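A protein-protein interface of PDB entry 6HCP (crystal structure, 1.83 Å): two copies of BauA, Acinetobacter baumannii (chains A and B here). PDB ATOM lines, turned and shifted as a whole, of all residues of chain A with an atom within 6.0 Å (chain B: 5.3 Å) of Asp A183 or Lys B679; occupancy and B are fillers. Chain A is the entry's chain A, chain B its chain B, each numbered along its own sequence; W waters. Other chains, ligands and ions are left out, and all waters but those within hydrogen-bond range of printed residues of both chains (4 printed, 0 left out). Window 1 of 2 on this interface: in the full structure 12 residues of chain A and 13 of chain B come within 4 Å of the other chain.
Among the printed residues, pairs that only touch across the chains: Phe A186 with Thr B650, Asp A183 with Thr B650 and Ala A184 with Thr B650.
Ser A182 touches none of the printed residues of chain B. Asp A183 touches just these residues of chain B: Thr B650 (3.8 Å) and Lys B679 (3.0 Å). Printed residues of chain B within 4 Å of Ala A184: Thr B650 (3.8 Å). Printed residues of chain B within 4 Å of Phe A186: Thr B650. Printed residues of chain A within 4 Å of Thr B650: Asp A183 (3.8 Å), Ala A184 (3.8 Å) and Phe A186 (3.7 Å). Lys B679 touches one residue of chain A. Ala B680 touches none of the printed residues of chain A. The nearest residue of chain B that does not touch Asp A183 is Thr B677 (4.9 Å). The nearest printed residue of chain B that does not touch Phe A186 is Arg B649 (7.0 Å).
The backbone NH of Asp A183 is in hydrogen-bond range of the backbone carbonyl oxygen of Asp A214 (3.3 Å). The backbone NH (N) of Asp A183 is in hydrogen-bond range of the backbone carbonyl oxygen (O) of Ala A215, 3.1 Å away. The backbone carbonyl oxygen (O) of Asp A214 sits at hydrogen-bond distance from the backbone NH (N) of Ala A184 (2.9 Å). The side-chain amide oxygen (OD1) of Asn B675 sits at hydrogen-bond distance from the backbone NH (N) of Lys B679 (3.1 Å).
OD2 of Asp A183 lies within salt-bridge range of NZ of Lys B679, 3.0 Å away.
Hydrophobic or aromatic side chains of chain A within 4 Å of the printed part of chain B: Ala A184 and Phe A186. Printed residues of chain B that touch a printed residue of chain A: Thr B650 and Lys B679. Among the printed residues, 4 pairs touch across the chains. Among the printed residues, Asp or Glu carboxylates within 4 Å of a Lys or Arg side-chain nitrogen of the other chain: Asp A183 with Lys B679.
Water W2 lies within hydrogen-bond range of OG1 of Thr B677 (2.5 Å) and OD1 of Asp A183 (2.7 Å). Water W3 lies within hydrogen-bond range of the backbone carbonyl oxygen of Asp A183 (2.5 Å), the side-chain hydroxyl of Tyr A180 (2.7 Å) and the backbone carbonyl oxygen of Thr B650 (2.9 Å). Water W1 lies within hydrogen-bond range of the side-chain carboxylate (OD2) of Asp A214 (2.6 Å) and the side-chain amino group (NZ) of Lys B679 (3.5 Å). Water W4 bridges the backbone NH of Thr B650 and the backbone carbonyl oxygen of Asp A183.
No position is printed for both chains. Of the 4 pairs that touch across the chains among the printed residues, none has its exchanged pair printed and touching as well.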
ATOM      1  N   TYR A 180      -4.347 -18.293  28.857  1.00  0.00           N
ATOM      2  CA  TYR A 180      -4.390 -19.543  28.147  1.00  0.00           C
ATOM      3  C   TYR A 180      -5.765 -19.665  27.466  1.00  0.00           C
ATOM      4  O   TYR A 180      -6.795 -19.301  28.037  1.00  0.00           O
ATOM      5  CB  TYR A 180      -4.153 -20.706  29.122  1.00  0.00           C
ATOM      6  CG  TYR A 180      -4.620 -22.049  28.642  1.00  0.00           C
ATOM      7  CD1 TYR A 180      -3.814 -22.876  27.885  1.00  0.00           C
ATOM      8  CD2 TYR A 180      -5.900 -22.483  28.926  1.00  0.00           C
ATOM      9  CE1 TYR A 180      -4.267 -24.107  27.435  1.00  0.00           C
ATOM     10  CE2 TYR A 180      -6.365 -23.707  28.487  1.00  0.00           C
ATOM     11  CZ  TYR A 180      -5.537 -24.536  27.760  1.00  0.00           C
ATOM     12  OH  TYR A 180      -6.059 -25.726  27.327  1.00  0.00           O
ATOM     13  N   MET A 181      -5.744 -20.238  26.266  1.00  0.00           N
ATOM     14  CA  MET A 181      -6.942 -20.700  25.619  1.00  0.00           C
ATOM     15  C   MET A 181      -6.633 -22.055  24.988  1.00  0.00           C
ATOM     16  O   MET A 181      -5.570 -22.263  24.424  1.00  0.00           O
ATOM     17  CB  MET A 181      -7.428 -19.711  24.546  1.00  0.00           C
ATOM     18  CG  MET A 181      -8.646 -20.209  23.787  1.00  0.00           C
ATOM     19  SD  MET A 181      -9.420 -18.908  22.743  1.00  0.00           S
ATOM     20  CE  MET A 181      -8.089 -18.433  21.651  1.00  0.00           C
ATOM     21  N   SER A 182      -7.558 -23.003  25.136  1.00  0.00           N
ATOM     22  CA  SER A 182      -7.357 -24.339  24.580  1.00  0.00           C
ATOM     23  C   SER A 182      -7.240 -24.252  23.058  1.00  0.00           C
ATOM     24  O   SER A 182      -7.802 -23.329  22.443  1.00  0.00           O
ATOM     25  CB  SER A 182      -8.466 -25.265  25.017  1.00  0.00           C
ATOM     26  OG  SER A 182      -9.737 -24.833  24.557  1.00  0.00           O
ATOM     27  N   ASP A 183      -6.435 -25.130  22.446  1.00  0.00           N
ATOM     28  CA  ASP A 183      -5.710 -26.223  23.091  1.00  0.00           C
ATOM     29  C   ASP A 183      -4.365 -25.760  23.678  1.00  0.00           C
ATOM     30  O   ASP A 183      -3.827 -26.427  24.575  1.00  0.00           O
ATOM     31  CB  ASP A 183      -5.447 -27.347  22.090  1.00  0.00           C
ATOM     32  CG  ASP A 183      -6.651 -28.220  21.802  1.00  0.00           C
ATOM     33  OD1 ASP A 183      -7.555 -28.204  22.625  1.00  0.00           O
ATOM     34  OD2 ASP A 183      -6.633 -28.923  20.771  1.00  0.00           O
ATOM     35  N   ALA A 184      -3.691 -24.790  23.053  1.00  0.00           N
ATOM     36  CA  ALA A 184      -2.327 -24.425  23.498  1.00  0.00           C
ATOM     37  C   ALA A 184      -1.970 -22.973  23.161  1.00  0.00           C
ATOM     38  O   ALA A 184      -0.859 -22.696  22.709  1.00  0.00           O
ATOM     39  CB  ALA A 184      -1.314 -25.391  22.915  1.00  0.00           C
ATOM     40  N   GLN A 185      -2.920 -22.054  23.350  1.00  0.00           N
ATOM     41  CA  GLN A 185      -2.642 -20.647  23.097  1.00  0.00           C
ATOM     42  C   GLN A 185      -2.248 -19.970  24.408  1.00  0.00           C
ATOM     43  O   GLN A 185      -3.021 -19.934  25.346  1.00  0.00           O
ATOM     44  CB  GLN A 185      -3.841 -19.902  22.508  1.00  0.00           C
ATOM     45  CG  GLN A 185      -3.415 -18.561  21.925  1.00  0.00           C
ATOM     46  CD  GLN A 185      -4.544 -17.572  21.806  1.00  0.00           C
ATOM     47  OE1 GLN A 185      -5.234 -17.285  22.782  1.00  0.00           O
ATOM     48  NE2 GLN A 185      -4.679 -16.998  20.612  1.00  0.00           N
ATOM     49  N   PHE A 186      -1.042 -19.403  24.434  1.00  0.00           N
ATOM     50  CA  PHE A 186      -0.562 -18.711  25.605  1.00  0.00           C
ATOM     51  C   PHE A 186      -0.332 -17.243  25.265  1.00  0.00           C
ATOM     52  O   PHE A 186       0.163 -16.930  24.195  1.00  0.00           O
ATOM     53  CB  PHE A 186       0.752 -19.318  26.099  1.00  0.00           C
ATOM     54  CG  PHE A 186       0.577 -20.714  26.630  1.00  0.00           C
ATOM     55  CD1 PHE A 186       0.121 -20.918  27.924  1.00  0.00           C
ATOM     56  CD2 PHE A 186       0.775 -21.802  25.807  1.00  0.00           C
ATOM     57  CE1 PHE A 186      -0.114 -22.205  28.390  1.00  0.00           C
ATOM     58  CE2 PHE A 186       0.603 -23.088  26.298  1.00  0.00           C
ATOM     59  CZ  PHE A 186       0.123 -23.281  27.567  1.00  0.00           C
ATOM     60  N   ASP A 214      -1.980 -22.996  19.268  1.00  0.00           N
ATOM     61  CA  ASP A 214      -3.092 -23.797  18.823  1.00  0.00           C
ATOM     62  C   ASP A 214      -4.367 -23.364  19.528  1.00  0.00           C
ATOM     63  O   ASP A 214      -4.408 -23.240  20.745  1.00  0.00           O
ATOM     64  CB  ASP A 214      -2.855 -25.277  19.127  1.00  0.00           C
ATOM     65  CG  ASP A 214      -1.753 -25.889  18.299  1.00  0.00           C
ATOM     66  OD1 ASP A 214      -1.396 -25.290  17.276  1.00  0.00           O
ATOM     67  OD2 ASP A 214      -1.387 -27.027  18.598  1.00  0.00           O
ATOM     68  N   ALA A 215      -5.432 -23.236  18.742  1.00  0.00           N
ATOM     69  CA  ALA A 215      -6.747 -22.845  19.255  1.00  0.00           C
ATOM     70  C   ALA A 215      -7.610 -24.102  19.391  1.00  0.00           C
ATOM     71  O   ALA A 215      -7.087 -25.225  19.377  1.00  0.00           O
ATOM     72  CB  ALA A 215      -7.400 -21.839  18.320  1.00  0.00           C
ATOM     73  N   ALA A 216      -8.931 -23.909  19.521  1.00  0.00           N
ATOM     74  CA  ALA A 216      -9.814 -25.005  19.914  1.00  0.00           C
ATOM     75  C   ALA A 216     -10.262 -25.813  18.701  1.00  0.00           C
ATOM     76  O   ALA A 216     -10.702 -26.947  18.826  1.00  0.00           O
ATOM     77  CB  ALA A 216     -10.983 -24.479  20.689  1.00  0.00           C
ATOM     78  N   VAL A 217     -10.154 -25.228  17.509  1.00  0.00           N
ATOM     79  CA  VAL A 217     -10.467 -25.938  16.293  1.00  0.00           C
ATOM     80  C   VAL A 217      -9.253 -26.778  15.880  1.00  0.00           C
ATOM     81  O   VAL A 217      -8.123 -26.290  15.951  1.00  0.00           O
ATOM     82  CB  VAL A 217     -10.894 -24.939  15.197  1.00  0.00           C
ATOM     83  CG1 VAL A 217     -10.978 -25.566  13.815  1.00  0.00           C
ATOM     84  CG2 VAL A 217     -12.222 -24.291  15.565  1.00  0.00           C
ATOM     85  N   ASN A 218      -9.499 -27.949  15.278  1.00  0.00           N
ATOM     86  CA  ASN A 218      -8.404 -28.788  14.747  1.00  0.00           C
ATOM     87  C   ASN A 218      -7.545 -27.993  13.756  1.00  0.00           C
ATOM     88  O   ASN A 218      -8.068 -27.382  12.831  1.00  0.00           O
ATOM     89  CB  ASN A 218      -8.903 -30.036  14.024  1.00  0.00           C
ATOM     90  CG  ASN A 218      -9.591 -31.040  14.929  1.00  0.00           C
ATOM     91  OD1 ASN A 218      -9.462 -30.990  16.148  1.00  0.00           O
ATOM     92  ND2 ASN A 218     -10.338 -31.954  14.334  1.00  0.00           N
ATOM     93  N   ALA B 272      -9.042 -39.438  21.582  1.00  0.00           N
ATOM     94  CA  ALA B 272      -7.999 -39.839  22.534  1.00  0.00           C
ATOM     95  C   ALA B 272      -8.295 -41.203  23.168  1.00  0.00           C
ATOM     96  O   ALA B 272      -7.369 -41.873  23.606  1.00  0.00           O
ATOM     97  CB  ALA B 272      -7.846 -38.776  23.599  1.00  0.00           C
ATOM     98  N   ARG B 649       2.121 -30.445  22.809  1.00  0.00           N
ATOM     99  CA  ARG B 649       0.770 -30.396  23.350  1.00  0.00           C
ATOM    100  C   ARG B 649       0.816 -29.900  24.795  1.00  0.00           C
ATOM    101  O   ARG B 649       1.855 -29.954  25.467  1.00  0.00           O
ATOM    102  CB  ARG B 649       0.039 -31.734  23.195  1.00  0.00           C
ATOM    103  CG  ARG B 649       0.164 -32.730  24.342  1.00  0.00           C
ATOM    104  CD  ARG B 649       1.488 -33.464  24.401  1.00  0.00           C
ATOM    105  NE  ARG B 649       1.892 -34.082  23.145  1.00  0.00           N
ATOM    106  CZ  ARG B 649       2.986 -34.840  22.972  1.00  0.00           C
ATOM    107  NH1 ARG B 649       3.265 -35.261  21.751  1.00  0.00           N
ATOM    108  NH2 ARG B 649       3.725 -35.248  24.009  1.00  0.00           N
ATOM    109  N   THR B 650      -0.334 -29.406  25.242  1.00  0.00           N
ATOM    110  CA  THR B 650      -0.538 -28.925  26.580  1.00  0.00           C
ATOM    111  C   THR B 650      -1.691 -29.704  27.188  1.00  0.00           C
ATOM    112  O   THR B 650      -2.767 -29.792  26.609  1.00  0.00           O
ATOM    113  CB  THR B 650      -0.811 -27.407  26.582  1.00  0.00           C
ATOM    114  OG1 THR B 650       0.357 -26.753  26.079  1.00  0.00           O
ATOM    115  CG2 THR B 650      -1.172 -26.877  27.951  1.00  0.00           C
ATOM    116  N   LEU B 651      -1.457 -30.273  28.370  1.00  0.00           N
ATOM    117  CA  LEU B 651      -2.433 -31.056  29.061  1.00  0.00           C
ATOM    118  C   LEU B 651      -2.750 -30.370  30.390  1.00  0.00           C
ATOM    119  O   LEU B 651      -1.820 -29.921  31.085  1.00  0.00           O
ATOM    120  CB  LEU B 651      -1.882 -32.472  29.291  1.00  0.00           C
ATOM    121  CG  LEU B 651      -1.472 -33.238  28.042  1.00  0.00           C
ATOM    122  CD1 LEU B 651      -0.938 -34.631  28.398  1.00  0.00           C
ATOM    123  CD2 LEU B 651      -2.645 -33.340  27.071  1.00  0.00           C
ATOM    124  N   ASN B 675      -6.005 -35.040  31.952  1.00  0.00           N
ATOM    125  CA  ASN B 675      -6.252 -34.677  30.560  1.00  0.00           C
ATOM    126  C   ASN B 675      -7.702 -34.177  30.432  1.00  0.00           C
ATOM    127  O   ASN B 675      -8.529 -34.749  29.689  1.00  0.00           O
ATOM    128  CB  ASN B 675      -5.960 -35.816  29.576  1.00  0.00           C
ATOM    129  CG  ASN B 675      -6.016 -35.343  28.137  1.00  0.00           C
ATOM    130  OD1 ASN B 675      -6.102 -34.134  27.879  1.00  0.00           O
ATOM    131  ND2 ASN B 675      -5.879 -36.263  27.194  1.00  0.00           N
ATOM    132  N   THR B 677      -9.178 -31.681  29.117  1.00  0.00           N
ATOM    133  CA  THR B 677      -9.668 -31.248  27.783  1.00  0.00           C
ATOM    134  C   THR B 677      -9.807 -32.431  26.806  1.00  0.00           C
ATOM    135  O   THR B 677     -10.324 -32.261  25.712  1.00  0.00           O
ATOM    136  CB  THR B 677      -8.772 -30.195  27.126  1.00  0.00           C
ATOM    137  OG1 THR B 677      -7.518 -30.762  26.750  1.00  0.00           O
ATOM    138  CG2 THR B 677      -8.521 -28.971  27.985  1.00  0.00           C
ATOM    139  N   ASN B 678      -9.356 -33.627  27.201  1.00  0.00           N
ATOM    140  CA  ASN B 678      -9.430 -34.813  26.359  1.00  0.00           C
ATOM    141  C   ASN B 678      -8.685 -34.587  25.041  1.00  0.00           C
ATOM    142  O   ASN B 678      -9.108 -35.067  23.974  1.00  0.00           O
ATOM    143  CB  ASN B 678     -10.875 -35.231  26.099  1.00  0.00           C
ATOM    144  CG  ASN B 678     -11.026 -36.700  25.795  1.00  0.00           C
ATOM    145  OD1 ASN B 678     -10.181 -37.510  26.160  1.00  0.00           O
ATOM    146  ND2 ASN B 678     -12.055 -37.041  25.044  1.00  0.00           N
ATOM    147  N   LYS B 679      -7.493 -34.013  25.141  1.00  0.00           N
ATOM    148  CA  LYS B 679      -6.647 -33.799  23.997  1.00  0.00           C
ATOM    149  C   LYS B 679      -6.177 -35.135  23.399  1.00  0.00           C
ATOM    150  O   LYS B 679      -5.539 -35.952  24.088  1.00  0.00           O
ATOM    151  CB  LYS B 679      -5.433 -32.967  24.407  1.00  0.00           C
ATOM    152  CG  LYS B 679      -4.435 -32.654  23.305  1.00  0.00           C
ATOM    153  CD  LYS B 679      -4.978 -31.796  22.172  1.00  0.00           C
ATOM    154  CE  LYS B 679      -3.911 -31.447  21.154  1.00  0.00           C
ATOM    155  NZ  LYS B 679      -4.520 -30.916  19.912  1.00  0.00           N
ATOM    156  N   ALA B 680      -6.345 -35.257  22.080  1.00  0.00           N
ATOM    157  CA  ALA B 680      -5.794 -36.352  21.267  1.00  0.00           C
ATOM    158  C   ALA B 680      -4.408 -35.960  20.786  1.00  0.00           C
ATOM    159  O   ALA B 680      -4.258 -34.951  20.088  1.00  0.00           O
ATOM    160  CB  ALA B 680      -6.681 -36.623  20.079  1.00  0.00           C
ATOM    161  N   TYR B 681      -3.394 -36.788  21.088  1.00  0.00           N
ATOM    162  CA  TYR B 681      -2.057 -36.530  20.596  1.00  0.00           C
ATOM    163  C   TYR B 681      -1.282 -37.836  20.403  1.00  0.00           C
ATOM    164  O   TYR B 681      -1.541 -38.826  21.089  1.00  0.00           O
ATOM    165  CB  TYR B 681      -1.270 -35.610  21.546  1.00  0.00           C
ATOM    166  CG  TYR B 681      -1.017 -36.186  22.915  1.00  0.00           C
ATOM    167  CD1 TYR B 681      -1.949 -36.051  23.931  1.00  0.00           C
ATOM    168  CD2 TYR B 681       0.177 -36.829  23.212  1.00  0.00           C
ATOM    169  CE1 TYR B 681      -1.744 -36.610  25.183  1.00  0.00           C
ATOM    170  CE2 TYR B 681       0.410 -37.371  24.465  1.00  0.00           C
ATOM    171  CZ  TYR B 681      -0.542 -37.241  25.459  1.00  0.00           C
ATOM    172  OH  TYR B 681      -0.344 -37.772  26.703  1.00  0.00           O
ATOM    173  N   GLY B 693      -1.782 -40.661  23.361  1.00  0.00           N
ATOM    174  CA  GLY B 693      -1.814 -40.310  24.766  1.00  0.00           C
ATOM    175  C   GLY B 693      -3.104 -40.719  25.438  1.00  0.00           C
ATOM    176  O   GLY B 693      -4.139 -40.784  24.802  1.00  0.00           O
ATOM    177  N   ALA B 694      -3.045 -40.905  26.762  1.00  0.00           N
ATOM    178  CA  ALA B 694      -4.181 -41.275  27.559  1.00  0.00           C
ATOM    179  C   ALA B 694      -5.276 -40.216  27.417  1.00  0.00           C
ATOM    180  O   ALA B 694      -4.996 -39.021  27.395  1.00  0.00           O
ATOM    181  CB  ALA B 694      -3.771 -41.424  29.010  1.00  0.00           C
HETATM  182  O   HOH W   1      -2.242 -28.427  20.668  1.00  0.00           O
HETATM  183  O   HOH W   2      -6.705 -29.299  24.919  1.00  0.00           O
HETATM  184  O   HOH W   3      -4.934 -27.971  26.236  1.00  0.00           O
HETATM  185  O   HOH W   4      -2.418 -29.128  23.360  1.00  0.00           O
